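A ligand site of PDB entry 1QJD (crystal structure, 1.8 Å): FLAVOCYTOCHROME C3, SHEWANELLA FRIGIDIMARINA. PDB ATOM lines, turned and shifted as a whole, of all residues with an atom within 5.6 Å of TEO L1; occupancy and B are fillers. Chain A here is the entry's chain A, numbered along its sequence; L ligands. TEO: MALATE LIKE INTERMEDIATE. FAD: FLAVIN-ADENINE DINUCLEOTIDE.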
ATOM      1  N   ALA A 168      -8.749   7.295  -1.381  1.00  0.00           N
ATOM      2  CA  ALA A 168      -8.408   8.673  -1.035  1.00  0.00           C
ATOM      3  C   ALA A 168      -8.274   9.538  -2.270  1.00  0.00           C
ATOM      4  O   ALA A 168      -7.769   9.036  -3.281  1.00  0.00           O
ATOM      5  CB  ALA A 168      -7.136   8.671  -0.191  1.00  0.00           C
ATOM      6  N   ALA A 169      -8.731  10.783  -2.211  1.00  0.00           N
ATOM      7  CA  ALA A 169      -8.722  11.632  -3.407  1.00  0.00           C
ATOM      8  C   ALA A 169      -7.880  12.900  -3.247  1.00  0.00           C
ATOM      9  O   ALA A 169      -6.843  13.053  -3.918  1.00  0.00           O
ATOM     10  CB  ALA A 169     -10.151  11.993  -3.770  1.00  0.00           C
ATOM     11  N   GLY A 170      -8.319  13.793  -2.379  1.00  0.00           N
ATOM     12  CA  GLY A 170      -7.890  15.150  -2.209  1.00  0.00           C
ATOM     13  C   GLY A 170      -6.428  15.358  -1.888  1.00  0.00           C
ATOM     14  O   GLY A 170      -5.856  16.390  -2.272  1.00  0.00           O
ATOM     15  N   GLY A 171      -5.791  14.424  -1.179  1.00  0.00           N
ATOM     16  CA  GLY A 171      -4.374  14.473  -0.940  1.00  0.00           C
ATOM     17  C   GLY A 171      -3.913  14.177   0.470  1.00  0.00           C
ATOM     18  O   GLY A 171      -4.676  13.857   1.377  1.00  0.00           O
ATOM     19  N   MET A 236      -7.402  22.323   1.034  1.00  0.00           N
ATOM     20  CA  MET A 236      -8.553  21.595   1.563  1.00  0.00           C
ATOM     21  C   MET A 236      -9.183  22.445   2.649  1.00  0.00           C
ATOM     22  O   MET A 236      -8.587  23.444   3.049  1.00  0.00           O
ATOM     23  CB  MET A 236      -8.147  20.213   2.054  1.00  0.00           C
ATOM     24  CG  MET A 236      -7.539  19.360   0.929  1.00  0.00           C
ATOM     25  SD  MET A 236      -8.854  18.596  -0.057  1.00  0.00           S
ATOM     26  CE  MET A 236      -9.243  17.228   1.050  1.00  0.00           C
ATOM     27  N   GLN A 363     -16.849  11.931  11.926  1.00  0.00           N
ATOM     28  CA  GLN A 363     -16.881  12.939  10.880  1.00  0.00           C
ATOM     29  C   GLN A 363     -17.741  12.547   9.706  1.00  0.00           C
ATOM     30  O   GLN A 363     -17.682  11.475   9.102  1.00  0.00           O
ATOM     31  CB  GLN A 363     -15.446  13.256  10.406  1.00  0.00           C
ATOM     32  CG  GLN A 363     -15.478  14.063   9.096  1.00  0.00           C
ATOM     33  CD  GLN A 363     -14.083  14.603   8.842  1.00  0.00           C
ATOM     34  OE1 GLN A 363     -13.363  14.013   8.039  1.00  0.00           O
ATOM     35  NE2 GLN A 363     -13.722  15.686   9.532  1.00  0.00           N
ATOM     36  N   HIS A 365     -18.416  13.487   5.866  1.00  0.00           N
ATOM     37  CA  HIS A 365     -17.929  14.254   4.720  1.00  0.00           C
ATOM     38  C   HIS A 365     -19.107  15.096   4.205  1.00  0.00           C
ATOM     39  O   HIS A 365     -20.198  14.559   4.076  1.00  0.00           O
ATOM     40  CB  HIS A 365     -17.422  13.333   3.624  1.00  0.00           C
ATOM     41  CG  HIS A 365     -16.600  14.008   2.577  1.00  0.00           C
ATOM     42  ND1 HIS A 365     -17.114  14.898   1.653  1.00  0.00           N
ATOM     43  CD2 HIS A 365     -15.272  13.903   2.333  1.00  0.00           C
ATOM     44  CE1 HIS A 365     -16.124  15.315   0.879  1.00  0.00           C
ATOM     45  NE2 HIS A 365     -14.996  14.726   1.271  1.00  0.00           N
ATOM     46  N   MET A 375     -18.198   9.382  -2.346  1.00  0.00           N
ATOM     47  CA  MET A 375     -17.611  10.641  -1.929  1.00  0.00           C
ATOM     48  C   MET A 375     -17.198  11.489  -3.136  1.00  0.00           C
ATOM     49  O   MET A 375     -16.597  10.926  -4.059  1.00  0.00           O
ATOM     50  CB  MET A 375     -16.385  10.361  -1.059  1.00  0.00           C
ATOM     51  CG  MET A 375     -15.857  11.591  -0.332  1.00  0.00           C
ATOM     52  SD  MET A 375     -14.663  12.474  -1.390  1.00  0.00           S
ATOM     53  CE  MET A 375     -13.421  11.192  -1.592  1.00  0.00           C
ATOM     54  N   VAL A 376     -17.505  12.780  -3.129  1.00  0.00           N
ATOM     55  CA  VAL A 376     -16.948  13.718  -4.102  1.00  0.00           C
ATOM     56  C   VAL A 376     -15.905  14.594  -3.431  1.00  0.00           C
ATOM     57  O   VAL A 376     -16.204  15.331  -2.496  1.00  0.00           O
ATOM     58  CB  VAL A 376     -18.058  14.616  -4.700  1.00  0.00           C
ATOM     59  CG1 VAL A 376     -17.471  15.692  -5.595  1.00  0.00           C
ATOM     60  CG2 VAL A 376     -19.044  13.753  -5.487  1.00  0.00           C
ATOM     61  N   THR A 377     -14.638  14.594  -3.841  1.00  0.00           N
ATOM     62  CA  THR A 377     -13.581  15.212  -3.073  1.00  0.00           C
ATOM     63  C   THR A 377     -13.765  16.707  -2.812  1.00  0.00           C
ATOM     64  O   THR A 377     -14.223  17.555  -3.585  1.00  0.00           O
ATOM     65  CB  THR A 377     -12.205  14.989  -3.745  1.00  0.00           C
ATOM     66  OG1 THR A 377     -11.201  15.621  -2.946  1.00  0.00           O
ATOM     67  CG2 THR A 377     -12.117  15.596  -5.135  1.00  0.00           C
ATOM     68  N   GLU A 378     -13.348  17.033  -1.604  1.00  0.00           N
ATOM     69  CA  GLU A 378     -13.247  18.389  -1.078  1.00  0.00           C
ATOM     70  C   GLU A 378     -12.301  19.201  -1.954  1.00  0.00           C
ATOM     71  O   GLU A 378     -12.379  20.415  -2.012  1.00  0.00           O
ATOM     72  CB  GLU A 378     -12.774  18.311   0.367  1.00  0.00           C
ATOM     73  CG  GLU A 378     -12.573  19.630   1.094  1.00  0.00           C
ATOM     74  CD  GLU A 378     -12.773  19.477   2.600  1.00  0.00           C
ATOM     75  OE1 GLU A 378     -13.822  18.905   2.973  1.00  0.00           O
ATOM     76  OE2 GLU A 378     -11.912  19.927   3.370  1.00  0.00           O
ATOM     77  N   ALA A 379     -11.378  18.519  -2.657  1.00  0.00           N
ATOM     78  CA  ALA A 379     -10.492  19.257  -3.564  1.00  0.00           C
ATOM     79  C   ALA A 379     -11.288  19.932  -4.679  1.00  0.00           C
ATOM     80  O   ALA A 379     -10.833  20.900  -5.294  1.00  0.00           O
ATOM     81  CB  ALA A 379      -9.455  18.319  -4.133  1.00  0.00           C
ATOM     82  N   ARG A 402     -15.372  20.592   8.157  1.00  0.00           N
ATOM     83  CA  ARG A 402     -16.425  19.699   7.686  1.00  0.00           C
ATOM     84  C   ARG A 402     -17.646  19.657   8.600  1.00  0.00           C
ATOM     85  O   ARG A 402     -18.734  19.345   8.132  1.00  0.00           O
ATOM     86  CB  ARG A 402     -15.872  18.260   7.533  1.00  0.00           C
ATOM     87  CG  ARG A 402     -15.000  18.169   6.299  1.00  0.00           C
ATOM     88  CD  ARG A 402     -14.346  16.816   6.103  1.00  0.00           C
ATOM     89  NE  ARG A 402     -13.641  16.789   4.836  1.00  0.00           N
ATOM     90  CZ  ARG A 402     -12.742  15.876   4.479  1.00  0.00           C
ATOM     91  NH1 ARG A 402     -12.403  14.864   5.265  1.00  0.00           N
ATOM     92  NH2 ARG A 402     -12.193  16.006   3.278  1.00  0.00           N
ATOM     93  N   HIS A 504     -18.010   9.370   7.238  1.00  0.00           N
ATOM     94  CA  HIS A 504     -16.748   9.212   6.504  1.00  0.00           C
ATOM     95  C   HIS A 504     -15.570   8.678   7.292  1.00  0.00           C
ATOM     96  O   HIS A 504     -14.798   7.863   6.769  1.00  0.00           O
ATOM     97  CB  HIS A 504     -16.370  10.627   6.013  1.00  0.00           C
ATOM     98  CG  HIS A 504     -15.203  10.704   5.071  1.00  0.00           C
ATOM     99  ND1 HIS A 504     -15.106  10.025   3.896  1.00  0.00           N
ATOM    100  CD2 HIS A 504     -14.084  11.473   5.164  1.00  0.00           C
ATOM    101  CE1 HIS A 504     -13.955  10.338   3.295  1.00  0.00           C
ATOM    102  NE2 HIS A 504     -13.324  11.215   4.043  1.00  0.00           N
ATOM    103  N   ARG A 544     -11.613  16.241  12.011  1.00  0.00           N
ATOM    104  CA  ARG A 544     -10.398  16.051  11.249  1.00  0.00           C
ATOM    105  C   ARG A 544     -10.323  16.947  10.010  1.00  0.00           C
ATOM    106  O   ARG A 544     -11.331  17.098   9.331  1.00  0.00           O
ATOM    107  CB  ARG A 544     -10.309  14.598  10.764  1.00  0.00           C
ATOM    108  CG  ARG A 544      -9.065  14.414   9.899  1.00  0.00           C
ATOM    109  CD  ARG A 544      -8.841  12.932   9.655  1.00  0.00           C
ATOM    110  NE  ARG A 544      -9.749  12.313   8.723  1.00  0.00           N
ATOM    111  CZ  ARG A 544      -9.819  12.546   7.420  1.00  0.00           C
ATOM    112  NH1 ARG A 544      -9.025  13.431   6.834  1.00  0.00           N
ATOM    113  NH2 ARG A 544     -10.704  11.873   6.675  1.00  0.00           N
ATOM    114  N   LEU A 545      -9.138  17.488   9.730  1.00  0.00           N
ATOM    115  CA  LEU A 545      -8.936  18.288   8.520  1.00  0.00           C
ATOM    116  C   LEU A 545      -8.784  17.402   7.295  1.00  0.00           C
ATOM    117  O   LEU A 545      -8.091  16.371   7.360  1.00  0.00           O
ATOM    118  CB  LEU A 545      -7.689  19.169   8.664  1.00  0.00           C
ATOM    119  CG  LEU A 545      -7.680  20.271   9.728  1.00  0.00           C
ATOM    120  CD1 LEU A 545      -6.423  21.136   9.592  1.00  0.00           C
ATOM    121  CD2 LEU A 545      -8.921  21.158   9.648  1.00  0.00           C
ATOM    122  N   GLY A 546      -9.398  17.808   6.179  1.00  0.00           N
ATOM    123  CA  GLY A 546      -9.184  17.040   4.947  1.00  0.00           C
ATOM    124  C   GLY A 546      -7.691  16.947   4.665  1.00  0.00           C
ATOM    125  O   GLY A 546      -7.003  17.952   4.806  1.00  0.00           O
ATOM    126  N   GLY A 547      -7.156  15.778   4.305  1.00  0.00           N
ATOM    127  CA  GLY A 547      -5.731  15.628   4.016  1.00  0.00           C
ATOM    128  C   GLY A 547      -4.931  15.134   5.199  1.00  0.00           C
ATOM    129  O   GLY A 547      -3.768  14.718   5.116  1.00  0.00           O
ATOM    130  N   ASN A 548      -5.558  15.163   6.387  1.00  0.00           N
ATOM    131  CA  ASN A 548      -4.716  14.816   7.543  1.00  0.00           C
ATOM    132  C   ASN A 548      -4.727  13.313   7.850  1.00  0.00           C
ATOM    133  O   ASN A 548      -3.902  12.839   8.653  1.00  0.00           O
ATOM    134  CB  ASN A 548      -5.172  15.640   8.748  1.00  0.00           C
ATOM    135  CG  ASN A 548      -4.308  16.853   9.036  1.00  0.00           C
ATOM    136  OD1 ASN A 548      -3.416  17.229   8.267  1.00  0.00           O
ATOM    137  ND2 ASN A 548      -4.527  17.494  10.189  1.00  0.00           N
ATOM    138  N   ALA A 549      -5.630  12.555   7.259  1.00  0.00           N
ATOM    139  CA  ALA A 549      -5.693  11.115   7.575  1.00  0.00           C
ATOM    140  C   ALA A 549      -4.650  10.341   6.801  1.00  0.00           C
ATOM    141  O   ALA A 549      -3.978   9.435   7.311  1.00  0.00           O
ATOM    142  CB  ALA A 549      -7.096  10.604   7.305  1.00  0.00           C
HETATM  143  C1  TEO L   1     -11.425  14.387   0.036  1.00  0.00           C
HETATM  144  O1A TEO L   1     -10.789  14.038  -0.885  1.00  0.00           O
HETATM  145  O1B TEO L   1     -12.381  15.134   0.161  1.00  0.00           O
HETATM  146  C2  TEO L   1     -11.260  13.526   1.385  1.00  0.00           C
HETATM  147  O2  TEO L   1     -12.327  12.840   1.725  1.00  0.00           O
HETATM  148  C3  TEO L   1     -10.239  14.050   2.133  1.00  0.00           C
HETATM  149  C4  TEO L   1     -10.098  13.677   3.442  1.00  0.00           C
HETATM  150  O4A TEO L   1      -9.096  13.845   4.284  1.00  0.00           O
HETATM  151  O4B TEO L   1     -11.037  12.701   4.051  1.00  0.00           O
HETATM  152  PA  FAD L   2      -7.678   1.494   5.920  1.00  0.00           P
HETATM  153  O1A FAD L   2      -9.139   1.467   6.014  1.00  0.00           O
HETATM  154  O2A FAD L   2      -6.986   2.083   4.746  1.00  0.00           O
HETATM  155  O5B FAD L   2      -7.134  -0.015   5.978  1.00  0.00           O
HETATM  156  C5B FAD L   2      -7.473  -0.889   7.070  1.00  0.00           C
HETATM  157  C4B FAD L   2      -7.560  -2.294   6.495  1.00  0.00           C
HETATM  158  O4B FAD L   2      -7.657  -3.170   7.634  1.00  0.00           O
HETATM  159  C3B FAD L   2      -8.773  -2.578   5.628  1.00  0.00           C
HETATM  160  O3B FAD L   2      -8.471  -3.090   4.355  1.00  0.00           O
HETATM  161  C2B FAD L   2      -9.627  -3.492   6.524  1.00  0.00           C
HETATM  162  O2B FAD L   2     -10.376  -4.399   5.744  1.00  0.00           O
HETATM  163  C1B FAD L   2      -8.494  -4.237   7.301  1.00  0.00           C
HETATM  164  N9A FAD L   2      -8.965  -4.816   8.545  1.00  0.00           N
HETATM  165  C8A FAD L   2      -9.851  -4.344   9.498  1.00  0.00           C
HETATM  166  N7A FAD L   2     -10.010  -5.151  10.528  1.00  0.00           N
HETATM  167  C5A FAD L   2      -9.272  -6.274  10.178  1.00  0.00           C
HETATM  168  C6A FAD L   2      -8.941  -7.441  10.879  1.00  0.00           C
HETATM  169  N6A FAD L   2      -9.476  -7.722  12.065  1.00  0.00           N
HETATM  170  N1A FAD L   2      -8.106  -8.327  10.313  1.00  0.00           N
HETATM  171  C2A FAD L   2      -7.554  -8.031   9.117  1.00  0.00           C
HETATM  172  N3A FAD L   2      -7.767  -6.920   8.378  1.00  0.00           N
HETATM  173  C4A FAD L   2      -8.502  -6.018   9.075  1.00  0.00           C
HETATM  174  N1  FAD L   2      -7.957  11.116   4.107  1.00  0.00           N
HETATM  175  C2  FAD L   2      -7.045  12.046   3.676  1.00  0.00           C
HETATM  176  O2  FAD L   2      -6.217  12.551   4.444  1.00  0.00           O
HETATM  177  N3  FAD L   2      -6.956  12.442   2.342  1.00  0.00           N
HETATM  178  C4  FAD L   2      -7.811  11.985   1.319  1.00  0.00           C
HETATM  179  O4  FAD L   2      -7.774  12.338   0.195  1.00  0.00           O
HETATM  180  C4X FAD L   2      -8.875  11.063   1.822  1.00  0.00           C
HETATM  181  N5  FAD L   2      -9.706  10.583   0.946  1.00  0.00           N
HETATM  182  C5X FAD L   2     -10.655   9.699   1.416  1.00  0.00           C
HETATM  183  C6  FAD L   2     -11.635   9.189   0.489  1.00  0.00           C
HETATM  184  C7  FAD L   2     -12.531   8.188   0.871  1.00  0.00           C
HETATM  185  C7M FAD L   2     -13.625   7.690  -0.048  1.00  0.00           C
HETATM  186  C8  FAD L   2     -12.392   7.612   2.173  1.00  0.00           C
HETATM  187  C8M FAD L   2     -13.335   6.526   2.630  1.00  0.00           C
HETATM  188  C9  FAD L   2     -11.459   8.157   3.127  1.00  0.00           C
HETATM  189  C9A FAD L   2     -10.573   9.180   2.720  1.00  0.00           C
HETATM  190  N10 FAD L   2      -9.702   9.745   3.619  1.00  0.00           N
HETATM  191  C10 FAD L   2      -8.787  10.666   3.191  1.00  0.00           C
HETATM  192  C1' FAD L   2      -9.449   9.000   4.898  1.00  0.00           C
HETATM  193  C2' FAD L   2      -8.343   8.038   4.740  1.00  0.00           C
HETATM  194  O2' FAD L   2      -8.291   7.357   3.469  1.00  0.00           O
HETATM  195  C3' FAD L   2      -8.598   6.857   5.790  1.00  0.00           C
HETATM  196  O3' FAD L   2      -8.628   7.487   7.083  1.00  0.00           O
HETATM  197  C4' FAD L   2      -7.476   5.804   5.734  1.00  0.00           C
HETATM  198  O4' FAD L   2      -8.041   4.819   4.791  1.00  0.00           O
HETATM  199  C5' FAD L   2      -7.207   5.179   7.118  1.00  0.00           C
HETATM  200  O5' FAD L   2      -6.188   4.330   6.615  1.00  0.00           O
HETATM  201  P   FAD L   2      -5.825   3.088   7.558  1.00  0.00           P
HETATM  202  O1P FAD L   2      -4.584   2.472   7.011  1.00  0.00           O
HETATM  203  O2P FAD L   2      -5.875   3.483   8.956  1.00  0.00           O
HETATM  204  O3P FAD L   2      -7.048   2.122   7.235  1.00  0.00           O
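A nitrogen (N3) of FAD L2 lies close to an oxygen (O4A) of TEO L1, 3.2 Å away.
Residues that only touch TEO L1: Gly 546, Met 236, Ala 169 and Met 375.
NH1 of Arg 544 lies within hydrogen-bond range of O4A of TEO L1, at 2.6 Å.
The side-chain hydroxyl (OG1) of Thr 377 sits at hydrogen-bond distance from an oxygen (O1A) of TEO L1, at 2.6 Å.
NE2 of His 504 lies within hydrogen-bond range of O4B of TEO L1 (2.7 Å).
The backbone NH (N) of Gly 547 is in hydrogen-bond range of an oxygen (O4A) of TEO L1 (2.7 Å).
O1B of TEO L1 lies within hydrogen-bond range of N of Glu 378 (2.8 Å).
An oxygen (O1B) of TEO L1 is in salt-bridge range of the guanidinium group (NH2) of Arg 402, 3.2 Å away.
A ring nitrogen (NE2) of His 365 lies within hydrogen-bond range of an oxygen (O1B) of TEO L1.
The backbone NH (N) of Gly 170 sits at hydrogen-bond distance from an oxygen (O1A) of TEO L1, at 2.9 Å.
N of Gly 547 lies close to O2 of FAD L2 (3.4 Å).
The backbone NH (N) of Gly 170 sits at hydrogen-bond distance from an oxygen (O4) of FAD L2 (3.0 Å).
The backbone NH of Ala 169 sits at hydrogen-bond distance from an oxygen (O4) of FAD L2.
The backbone NH of Asn 548 sits at hydrogen-bond distance from an oxygen (O2) of FAD L2, 3.3 Å away.
The backbone NH (N) of Ala 549 is in hydrogen-bond range of an oxygen (O2) of FAD L2.
The backbone NH (N) of Gly 171 lies within hydrogen-bond range of an oxygen (O4) of FAD L2.
O of Gly 171 sits at hydrogen-bond distance from N3 of FAD L2, 2.9 Å away.
O of Arg 544 sits at hydrogen-bond distance from NE2 of Gln 363.
The backbone NH of Thr 377 sits at hydrogen-bond distance from the side-chain sulfur of Met 375 (3.2 Å).
OG1 of Thr 377 is in hydrogen-bond range of N of Ala 379 (2.9 Å).
The backbone NH (N) of His 504 is in hydrogen-bond range of the backbone carbonyl oxygen (O) of Gln 363 (2.8 Å).
NE of Arg 402 lies within salt-bridge range of OE1 of Glu 378, 2.8 Å away.
NH1 of Arg 402 is in hydrogen-bond range of OE1 of Gln 363 (3.1 Å).
A ring nitrogen (NE2) of His 365 lies within hydrogen-bond range of the side-chain sulfur of Met 375 (3.5 Å).
SD of Met 236 lies within hydrogen-bond range of N of Ala 379 (3.6 Å).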
